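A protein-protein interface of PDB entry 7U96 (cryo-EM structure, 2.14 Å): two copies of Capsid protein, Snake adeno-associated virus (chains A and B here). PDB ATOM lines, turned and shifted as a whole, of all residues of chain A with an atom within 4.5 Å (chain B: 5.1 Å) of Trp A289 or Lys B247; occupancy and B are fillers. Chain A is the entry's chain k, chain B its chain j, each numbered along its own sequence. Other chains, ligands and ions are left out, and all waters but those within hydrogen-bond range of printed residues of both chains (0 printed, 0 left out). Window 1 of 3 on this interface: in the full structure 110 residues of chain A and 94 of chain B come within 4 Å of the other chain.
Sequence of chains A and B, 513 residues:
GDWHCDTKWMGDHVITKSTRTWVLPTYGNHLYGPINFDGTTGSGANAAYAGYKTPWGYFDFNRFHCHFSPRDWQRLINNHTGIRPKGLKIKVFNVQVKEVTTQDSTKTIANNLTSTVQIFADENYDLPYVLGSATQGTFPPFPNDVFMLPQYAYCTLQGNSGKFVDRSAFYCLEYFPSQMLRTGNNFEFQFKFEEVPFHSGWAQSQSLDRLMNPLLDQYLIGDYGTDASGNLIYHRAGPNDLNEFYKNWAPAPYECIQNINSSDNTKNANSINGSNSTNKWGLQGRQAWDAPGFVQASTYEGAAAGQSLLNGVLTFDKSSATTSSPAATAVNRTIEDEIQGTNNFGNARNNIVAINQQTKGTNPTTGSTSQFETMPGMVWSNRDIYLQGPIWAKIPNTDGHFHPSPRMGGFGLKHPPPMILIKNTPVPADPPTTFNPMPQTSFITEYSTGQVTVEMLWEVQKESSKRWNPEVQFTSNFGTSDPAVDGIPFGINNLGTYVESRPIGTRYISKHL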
ATOM      1  N   SER A 275      -9.609  14.168  -1.396  1.00  0.00           N
ATOM      2  CA  SER A 275      -8.222  13.798  -1.635  1.00  0.00           C
ATOM      3  C   SER A 275      -7.979  12.328  -1.324  1.00  0.00           C
ATOM      4  O   SER A 275      -7.155  11.680  -1.975  1.00  0.00           O
ATOM      5  CB  SER A 275      -7.294  14.687  -0.813  1.00  0.00           C
ATOM      6  OG  SER A 275      -5.944  14.327  -1.028  1.00  0.00           O
ATOM      7  N   THR A 278      -9.559  10.124  -4.493  1.00  0.00           N
ATOM      8  CA  THR A 278      -9.161  10.294  -5.886  1.00  0.00           C
ATOM      9  C   THR A 278      -8.104   9.286  -6.316  1.00  0.00           C
ATOM     10  O   THR A 278      -7.380   8.721  -5.496  1.00  0.00           O
ATOM     11  CB  THR A 278      -8.652  11.712  -6.147  1.00  0.00           C
ATOM     12  OG1 THR A 278      -7.574  12.021  -5.258  1.00  0.00           O
ATOM     13  CG2 THR A 278      -9.751  12.692  -5.958  1.00  0.00           C
ATOM     14  N   ASN A 279      -8.028   9.061  -7.624  1.00  0.00           N
ATOM     15  CA  ASN A 279      -6.977   8.227  -8.188  1.00  0.00           C
ATOM     16  C   ASN A 279      -5.635   8.948  -8.173  1.00  0.00           C
ATOM     17  O   ASN A 279      -5.558  10.160  -8.378  1.00  0.00           O
ATOM     18  CB  ASN A 279      -7.323   7.813  -9.614  1.00  0.00           C
ATOM     19  CG  ASN A 279      -8.462   6.831  -9.676  1.00  0.00           C
ATOM     20  OD1 ASN A 279      -8.841   6.248  -8.672  1.00  0.00           O
ATOM     21  ND2 ASN A 279      -8.974   6.598 -10.867  1.00  0.00           N
ATOM     22  N   LYS A 280      -4.570   8.191  -7.933  1.00  0.00           N
ATOM     23  CA  LYS A 280      -3.244   8.759  -7.748  1.00  0.00           C
ATOM     24  C   LYS A 280      -2.202   7.898  -8.436  1.00  0.00           C
ATOM     25  O   LYS A 280      -2.332   6.677  -8.498  1.00  0.00           O
ATOM     26  CB  LYS A 280      -2.898   8.876  -6.262  1.00  0.00           C
ATOM     27  CG  LYS A 280      -3.771   9.843  -5.526  1.00  0.00           C
ATOM     28  CD  LYS A 280      -3.516   9.825  -4.052  1.00  0.00           C
ATOM     29  CE  LYS A 280      -4.417  10.813  -3.368  1.00  0.00           C
ATOM     30  NZ  LYS A 280      -4.287  10.727  -1.903  1.00  0.00           N
ATOM     31  N   TRP A 281      -1.151   8.542  -8.933  1.00  0.00           N
ATOM     32  CA  TRP A 281       0.038   7.818  -9.342  1.00  0.00           C
ATOM     33  C   TRP A 281       1.254   8.299  -8.566  1.00  0.00           C
ATOM     34  O   TRP A 281       1.347   9.463  -8.177  1.00  0.00           O
ATOM     35  CB  TRP A 281       0.297   7.891 -10.857  1.00  0.00           C
ATOM     36  CG  TRP A 281       0.278   9.228 -11.532  1.00  0.00           C
ATOM     37  CD1 TRP A 281      -0.731   9.746 -12.279  1.00  0.00           C
ATOM     38  CD2 TRP A 281       1.312  10.213 -11.519  1.00  0.00           C
ATOM     39  NE1 TRP A 281      -0.382  10.977 -12.755  1.00  0.00           N
ATOM     40  CE2 TRP A 281       0.869  11.292 -12.300  1.00  0.00           C
ATOM     41  CE3 TRP A 281       2.579  10.279 -10.941  1.00  0.00           C
ATOM     42  CZ2 TRP A 281       1.641  12.428 -12.510  1.00  0.00           C
ATOM     43  CZ3 TRP A 281       3.341  11.406 -11.147  1.00  0.00           C
ATOM     44  CH2 TRP A 281       2.870  12.466 -11.924  1.00  0.00           C
ATOM     45  N   ALA A 288       0.823  11.893  -6.612  1.00  0.00           N
ATOM     46  CA  ALA A 288       0.137  13.016  -7.225  1.00  0.00           C
ATOM     47  C   ALA A 288      -1.223  12.557  -7.719  1.00  0.00           C
ATOM     48  O   ALA A 288      -1.412  11.388  -8.048  1.00  0.00           O
ATOM     49  CB  ALA A 288       0.939  13.606  -8.385  1.00  0.00           C
ATOM     50  N   TRP A 289      -2.174  13.483  -7.772  1.00  0.00           N
ATOM     51  CA  TRP A 289      -3.489  13.148  -8.299  1.00  0.00           C
ATOM     52  C   TRP A 289      -3.387  12.761  -9.764  1.00  0.00           C
ATOM     53  O   TRP A 289      -2.641  13.373 -10.529  1.00  0.00           O
ATOM     54  CB  TRP A 289      -4.464  14.314  -8.168  1.00  0.00           C
ATOM     55  CG  TRP A 289      -4.912  14.644  -6.799  1.00  0.00           C
ATOM     56  CD1 TRP A 289      -4.415  14.163  -5.638  1.00  0.00           C
ATOM     57  CD2 TRP A 289      -6.033  15.455  -6.450  1.00  0.00           C
ATOM     58  NE1 TRP A 289      -5.118  14.667  -4.579  1.00  0.00           N
ATOM     59  CE2 TRP A 289      -6.127  15.456  -5.054  1.00  0.00           C
ATOM     60  CE3 TRP A 289      -6.961  16.192  -7.188  1.00  0.00           C
ATOM     61  CZ2 TRP A 289      -7.103  16.171  -4.376  1.00  0.00           C
ATOM     62  CZ3 TRP A 289      -7.922  16.904  -6.513  1.00  0.00           C
ATOM     63  CH2 TRP A 289      -7.987  16.888  -5.125  1.00  0.00           C
ATOM     64  N   ASP A 290      -4.154  11.751 -10.161  1.00  0.00           N
ATOM     65  CA  ASP A 290      -4.366  11.491 -11.580  1.00  0.00           C
ATOM     66  C   ASP A 290      -5.739  12.053 -11.946  1.00  0.00           C
ATOM     67  O   ASP A 290      -6.786  11.450 -11.724  1.00  0.00           O
ATOM     68  CB  ASP A 290      -4.257   9.995 -11.854  1.00  0.00           C
ATOM     69  CG  ASP A 290      -4.498   9.630 -13.311  1.00  0.00           C
ATOM     70  OD1 ASP A 290      -3.692  10.016 -14.176  1.00  0.00           O
ATOM     71  OD2 ASP A 290      -5.482   8.923 -13.594  1.00  0.00           O
ATOM     72  N   ALA A 291      -5.710  13.238 -12.533  1.00  0.00           N
ATOM     73  CA  ALA A 291      -6.933  13.926 -12.907  1.00  0.00           C
ATOM     74  C   ALA A 291      -6.682  14.773 -14.132  1.00  0.00           C
ATOM     75  O   ALA A 291      -5.640  15.395 -14.241  1.00  0.00           O
ATOM     76  CB  ALA A 291      -7.434  14.780 -11.766  1.00  0.00           C
ATOM     77  N   PRO A 292      -7.657  14.848 -15.037  1.00  0.00           N
ATOM     78  CA  PRO A 292      -8.941  14.147 -15.041  1.00  0.00           C
ATOM     79  C   PRO A 292      -8.805  12.649 -15.287  1.00  0.00           C
ATOM     80  O   PRO A 292      -9.763  11.916 -15.107  1.00  0.00           O
ATOM     81  CB  PRO A 292      -9.691  14.822 -16.179  1.00  0.00           C
ATOM     82  CG  PRO A 292      -8.625  15.233 -17.114  1.00  0.00           C
ATOM     83  CD  PRO A 292      -7.478  15.652 -16.256  1.00  0.00           C
ATOM     84  N   ASN A 311     -13.466  14.141  -9.811  1.00  0.00           N
ATOM     85  CA  ASN A 311     -12.273  14.588 -10.528  1.00  0.00           C
ATOM     86  C   ASN A 311     -12.086  13.858 -11.854  1.00  0.00           C
ATOM     87  O   ASN A 311     -10.961  13.577 -12.265  1.00  0.00           O
ATOM     88  CB  ASN A 311     -11.028  14.459  -9.655  1.00  0.00           C
ATOM     89  CG  ASN A 311     -11.024  15.451  -8.528  1.00  0.00           C
ATOM     90  OD1 ASN A 311     -10.892  15.097  -7.367  1.00  0.00           O
ATOM     91  ND2 ASN A 311     -11.159  16.714  -8.871  1.00  0.00           N
ATOM     92  N   ARG A 407      -4.387  14.608 -21.798  1.00  0.00           N
ATOM     93  CA  ARG A 407      -5.560  14.103 -21.095  1.00  0.00           C
ATOM     94  C   ARG A 407      -6.583  15.193 -20.813  1.00  0.00           C
ATOM     95  O   ARG A 407      -7.783  14.914 -20.753  1.00  0.00           O
ATOM     96  CB  ARG A 407      -5.157  13.408 -19.803  1.00  0.00           C
ATOM     97  CG  ARG A 407      -4.593  12.040 -20.028  1.00  0.00           C
ATOM     98  CD  ARG A 407      -4.418  11.319 -18.731  1.00  0.00           C
ATOM     99  NE  ARG A 407      -3.998   9.948 -18.944  1.00  0.00           N
ATOM    100  CZ  ARG A 407      -3.738   9.090 -17.969  1.00  0.00           C
ATOM    101  NH1 ARG A 407      -3.858   9.463 -16.711  1.00  0.00           N
ATOM    102  NH2 ARG A 407      -3.365   7.860 -18.261  1.00  0.00           N
ATOM    103  N   MET A 408      -6.145  16.439 -20.640  1.00  0.00           N
ATOM    104  CA  MET A 408      -7.114  17.500 -20.386  1.00  0.00           C
ATOM    105  C   MET A 408      -7.820  17.917 -21.670  1.00  0.00           C
ATOM    106  O   MET A 408      -8.961  18.380 -21.635  1.00  0.00           O
ATOM    107  CB  MET A 408      -6.437  18.690 -19.712  1.00  0.00           C
ATOM    108  CG  MET A 408      -5.916  18.379 -18.315  1.00  0.00           C
ATOM    109  SD  MET A 408      -5.271  19.775 -17.386  1.00  0.00           S
ATOM    110  CE  MET A 408      -3.681  20.046 -18.137  1.00  0.00           C
ATOM    111  N   LEU B 208       7.748  14.510 -13.660  1.00  0.00           N
ATOM    112  CA  LEU B 208       6.559  14.632 -14.487  1.00  0.00           C
ATOM    113  C   LEU B 208       5.388  15.231 -13.716  1.00  0.00           C
ATOM    114  O   LEU B 208       4.396  15.638 -14.322  1.00  0.00           O
ATOM    115  CB  LEU B 208       6.204  13.265 -15.050  1.00  0.00           C
ATOM    116  CG  LEU B 208       5.173  13.190 -16.156  1.00  0.00           C
ATOM    117  CD1 LEU B 208       5.748  13.846 -17.391  1.00  0.00           C
ATOM    118  CD2 LEU B 208       4.814  11.756 -16.424  1.00  0.00           C
ATOM    119  N   ASP B 209       5.473  15.301 -12.395  1.00  0.00           N
ATOM    120  CA  ASP B 209       4.436  15.972 -11.622  1.00  0.00           C
ATOM    121  C   ASP B 209       4.754  17.430 -11.305  1.00  0.00           C
ATOM    122  O   ASP B 209       3.938  18.096 -10.673  1.00  0.00           O
ATOM    123  CB  ASP B 209       4.174  15.218 -10.319  1.00  0.00           C
ATOM    124  CG  ASP B 209       5.425  15.022  -9.505  1.00  0.00           C
ATOM    125  OD1 ASP B 209       6.521  15.219 -10.055  1.00  0.00           O
ATOM    126  OD2 ASP B 209       5.320  14.710  -8.309  1.00  0.00           O
ATOM    127  N   MET B 212       4.618  22.301 -13.969  1.00  0.00           N
ATOM    128  CA  MET B 212       3.894  23.566 -13.896  1.00  0.00           C
ATOM    129  C   MET B 212       4.781  24.740 -13.475  1.00  0.00           C
ATOM    130  O   MET B 212       5.874  24.575 -12.933  1.00  0.00           O
ATOM    131  CB  MET B 212       2.744  23.436 -12.909  1.00  0.00           C
ATOM    132  CG  MET B 212       3.254  23.195 -11.517  1.00  0.00           C
ATOM    133  SD  MET B 212       2.045  22.387 -10.491  1.00  0.00           S
ATOM    134  CE  MET B 212       2.277  20.716 -11.036  1.00  0.00           C
ATOM    135  N   ASP B 223     -12.583  18.686  -7.441  1.00  0.00           N
ATOM    136  CA  ASP B 223     -13.618  18.230  -6.522  1.00  0.00           C
ATOM    137  C   ASP B 223     -12.998  17.900  -5.174  1.00  0.00           C
ATOM    138  O   ASP B 223     -12.200  16.968  -5.061  1.00  0.00           O
ATOM    139  CB  ASP B 223     -14.300  16.989  -7.084  1.00  0.00           C
ATOM    140  CG  ASP B 223     -15.065  17.264  -8.355  1.00  0.00           C
ATOM    141  OD1 ASP B 223     -15.395  18.435  -8.621  1.00  0.00           O
ATOM    142  OD2 ASP B 223     -15.320  16.302  -9.104  1.00  0.00           O
ATOM    143  N   LEU B 242       0.839  21.263  -4.950  1.00  0.00           N
ATOM    144  CA  LEU B 242       1.107  21.073  -6.369  1.00  0.00           C
ATOM    145  C   LEU B 242       0.700  19.681  -6.825  1.00  0.00           C
ATOM    146  O   LEU B 242       0.475  19.458  -8.019  1.00  0.00           O
ATOM    147  CB  LEU B 242       2.575  21.361  -6.689  1.00  0.00           C
ATOM    148  CG  LEU B 242       3.066  22.803  -6.539  1.00  0.00           C
ATOM    149  CD1 LEU B 242       4.540  22.888  -6.876  1.00  0.00           C
ATOM    150  CD2 LEU B 242       2.259  23.773  -7.386  1.00  0.00           C
ATOM    151  N   ASN B 243       0.532  18.759  -5.882  1.00  0.00           N
ATOM    152  CA  ASN B 243       0.163  17.386  -6.195  1.00  0.00           C
ATOM    153  C   ASN B 243      -1.270  17.251  -6.697  1.00  0.00           C
ATOM    154  O   ASN B 243      -1.616  16.217  -7.274  1.00  0.00           O
ATOM    155  CB  ASN B 243       0.384  16.507  -4.958  1.00  0.00           C
ATOM    156  CG  ASN B 243      -0.303  17.050  -3.724  1.00  0.00           C
ATOM    157  OD1 ASN B 243      -0.561  18.241  -3.619  1.00  0.00           O
ATOM    158  ND2 ASN B 243      -0.634  16.170  -2.800  1.00  0.00           N
ATOM    159  N   GLU B 244      -2.104  18.261  -6.493  1.00  0.00           N
ATOM    160  CA  GLU B 244      -3.513  18.192  -6.846  1.00  0.00           C
ATOM    161  C   GLU B 244      -3.832  18.845  -8.188  1.00  0.00           C
ATOM    162  O   GLU B 244      -4.999  18.880  -8.579  1.00  0.00           O
ATOM    163  CB  GLU B 244      -4.340  18.815  -5.728  1.00  0.00           C
ATOM    164  CG  GLU B 244      -4.084  18.114  -4.421  1.00  0.00           C
ATOM    165  CD  GLU B 244      -4.898  18.649  -3.266  1.00  0.00           C
ATOM    166  OE1 GLU B 244      -5.607  19.655  -3.425  1.00  0.00           O
ATOM    167  OE2 GLU B 244      -4.836  18.054  -2.178  1.00  0.00           O
ATOM    168  N   PHE B 245      -2.829  19.364  -8.885  1.00  0.00           N
ATOM    169  CA  PHE B 245      -3.004  19.886 -10.235  1.00  0.00           C
ATOM    170  C   PHE B 245      -3.508  18.822 -11.206  1.00  0.00           C
ATOM    171  O   PHE B 245      -3.015  17.695 -11.245  1.00  0.00           O
ATOM    172  CB  PHE B 245      -1.671  20.465 -10.723  1.00  0.00           C
ATOM    173  CG  PHE B 245      -1.367  21.840 -10.201  1.00  0.00           C
ATOM    174  CD1 PHE B 245      -1.264  22.906 -11.053  1.00  0.00           C
ATOM    175  CD2 PHE B 245      -1.301  22.082  -8.851  1.00  0.00           C
ATOM    176  CE1 PHE B 245      -0.996  24.165 -10.562  1.00  0.00           C
ATOM    177  CE2 PHE B 245      -1.064  23.316  -8.369  1.00  0.00           C
ATOM    178  CZ  PHE B 245      -0.915  24.367  -9.217  1.00  0.00           C
ATOM    179  N   TYR B 246      -4.494  19.208 -12.000  1.00  0.00           N
ATOM    180  CA  TYR B 246      -4.867  18.478 -13.202  1.00  0.00           C
ATOM    181  C   TYR B 246      -3.719  18.471 -14.207  1.00  0.00           C
ATOM    182  O   TYR B 246      -3.087  19.498 -14.456  1.00  0.00           O
ATOM    183  CB  TYR B 246      -6.110  19.129 -13.790  1.00  0.00           C
ATOM    184  CG  TYR B 246      -7.395  18.781 -13.073  1.00  0.00           C
ATOM    185  CD1 TYR B 246      -8.337  17.986 -13.680  1.00  0.00           C
ATOM    186  CD2 TYR B 246      -7.618  19.153 -11.757  1.00  0.00           C
ATOM    187  CE1 TYR B 246      -9.503  17.645 -13.045  1.00  0.00           C
ATOM    188  CE2 TYR B 246      -8.784  18.803 -11.103  1.00  0.00           C
ATOM    189  CZ  TYR B 246      -9.721  18.046 -11.754  1.00  0.00           C
ATOM    190  OH  TYR B 246     -10.883  17.694 -11.122  1.00  0.00           O
ATOM    191  N   LYS B 247      -3.442  17.309 -14.786  1.00  0.00           N
ATOM    192  CA  LYS B 247      -2.240  17.132 -15.584  1.00  0.00           C
ATOM    193  C   LYS B 247      -2.549  16.434 -16.899  1.00  0.00           C
ATOM    194  O   LYS B 247      -3.527  15.699 -17.019  1.00  0.00           O
ATOM    195  CB  LYS B 247      -1.185  16.363 -14.797  1.00  0.00           C
ATOM    196  CG  LYS B 247      -0.572  17.189 -13.687  1.00  0.00           C
ATOM    197  CD  LYS B 247       0.450  16.416 -12.887  1.00  0.00           C
ATOM    198  CE  LYS B 247      -0.188  15.385 -11.995  1.00  0.00           C
ATOM    199  NZ  LYS B 247      -0.964  16.008 -10.904  1.00  0.00           N
ATOM    200  N   ASN B 248      -1.715  16.717 -17.901  1.00  0.00           N
ATOM    201  CA  ASN B 248      -1.895  16.129 -19.226  1.00  0.00           C
ATOM    202  C   ASN B 248      -1.251  14.757 -19.356  1.00  0.00           C
ATOM    203  O   ASN B 248      -1.632  13.979 -20.233  1.00  0.00           O
ATOM    204  CB  ASN B 248      -1.336  17.062 -20.294  1.00  0.00           C
ATOM    205  CG  ASN B 248      -2.285  18.174 -20.642  1.00  0.00           C
ATOM    206  OD1 ASN B 248      -3.493  17.994 -20.625  1.00  0.00           O
ATOM    207  ND2 ASN B 248      -1.743  19.342 -20.914  1.00  0.00           N
ATOM    208  N   TRP B 249      -0.268  14.436 -18.527  1.00  0.00           N
ATOM    209  CA  TRP B 249       0.541  13.262 -18.801  1.00  0.00           C
ATOM    210  C   TRP B 249       0.725  12.426 -17.544  1.00  0.00           C
ATOM    211  O   TRP B 249       0.667  12.929 -16.425  1.00  0.00           O
ATOM    212  CB  TRP B 249       1.900  13.652 -19.385  1.00  0.00           C
ATOM    213  CG  TRP B 249       1.771  14.492 -20.597  1.00  0.00           C
ATOM    214  CD1 TRP B 249       2.100  15.798 -20.716  1.00  0.00           C
ATOM    215  CD2 TRP B 249       1.149  14.123 -21.828  1.00  0.00           C
ATOM    216  NE1 TRP B 249       1.797  16.249 -21.967  1.00  0.00           N
ATOM    217  CE2 TRP B 249       1.197  15.241 -22.668  1.00  0.00           C
ATOM    218  CE3 TRP B 249       0.578  12.951 -22.308  1.00  0.00           C
ATOM    219  CZ2 TRP B 249       0.699  15.220 -23.965  1.00  0.00           C
ATOM    220  CZ3 TRP B 249       0.083  12.932 -23.582  1.00  0.00           C
ATOM    221  CH2 TRP B 249       0.145  14.055 -24.400  1.00  0.00           C
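Of the 13 printed residues of chain A, 8 touch a printed residue of chain B.
Printed residues of chain A that touch a printed residue of chain B: Trp A281, Ala A288, Trp A289, Ala A291, Pro A292, Asn A311, Arg A407 and Met A408.
Hydrophobic or aromatic side chains of chain A within 4 Å of the printed part of chain B: Trp A281, Ala A288, Trp A289, Ala A291, Pro A292 and Met A408.
Of the 12 printed residues of chain B, 7 touch a printed residue of chain A.
Printed residues of chain B that touch a printed residue of chain A: Asp B209, Asp B223, Asn B243, Glu B244, Tyr B246, Lys B247 and Asn B248.
No position is printed for both chains.
NH1 of Arg A407 is in salt-bridge range of OD1 of Asp A290 (2.6 Å).
The backbone carbonyl oxygen (O) of Phe B245 is in hydrogen-bond range of the side-chain amino group (NZ) of Lys B247, 2.7 Å away.
O of Trp A281 is in hydrogen-bond range of N of Ala A288 (2.9 Å).
Asp B209 touches Trp A281 (CB to CH2, 3.4 Å).
Lys B247 touches Trp A281.
Asn B243 touches Ala A288.
Lys B247 touches Ala A288 (NZ to CB, 3.97 Å).
CE2 of Trp A289 touches CG of Glu B244, at 3.4 Å.
Tyr B246 touches Ala A291 (CA to O, 3.3 Å).
N of Pro A292 touches CD1 of Tyr B246 (3.5 Å).
CB of Arg A407 touches O of Lys B247, 3.96 Å away.
CG of Met A408 touches O of Lys B247, 3.8 Å away.
N of Met A408 sits at hydrogen-bond distance from OD1 of Asn B248 (3.1 Å).
O of Asn B248 is in hydrogen-bond range of N of Arg A407.
The backbone carbonyl oxygen of Tyr B246 sits close to the side-chain sulfur of Met A408 (3.7 Å).
The backbone NH (N) of Asp B223 lies close to the side-chain amide nitrogen (ND2) of Asn A311 (2.8 Å).
N of Trp A289 is in hydrogen-bond range of O of Asn B243 (2.8 Å).
NZ of Lys B247 lies within hydrogen-bond range of O of Trp A289 (3.1 Å).
The side-chain amide nitrogen of Asn A311 lies within hydrogen-bond range of the side-chain hydroxyl of Tyr B246, at 2.5 Å.
The backbone carbonyl oxygen (O) of Ala A291 is in hydrogen-bond range of the backbone NH (N) of Lys B247, 3.0 Å away.
Lys A280 touches none of the printed residues of chain B.
Of chain B, only Asn B243 (2.8 Å), Glu B244 (3.4 Å) and Lys B247 (3.1 Å) come within 4 Å of Trp A289.
Of the printed residues of chain B, Asn A311 touches Asp B223 and Tyr B246.
Printed residues of chain B within 4 Å of Arg A407: Lys B247 (3.96 Å) and Asn B248 (3.2 Å).
Of the printed residues of chain B, Met A408 touches Tyr B246, Lys B247 and Asn B248.
Phe B245 touches none of the printed residues of chain A.
Of the printed residues of chain A, Lys B247 touches Trp A281, Ala A288, Trp A289, Ala A291, Arg A407 and Met A408.
Printed residues of chain A within 4 Å of Asn B248: Arg A407 and Met A408.
The nearest residue of chain B that does not touch Trp A289 is Asp B223 (4.2 Å).
The nearest residue of chain A that does not touch Lys B247 is Pro A292 (4.02 Å).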
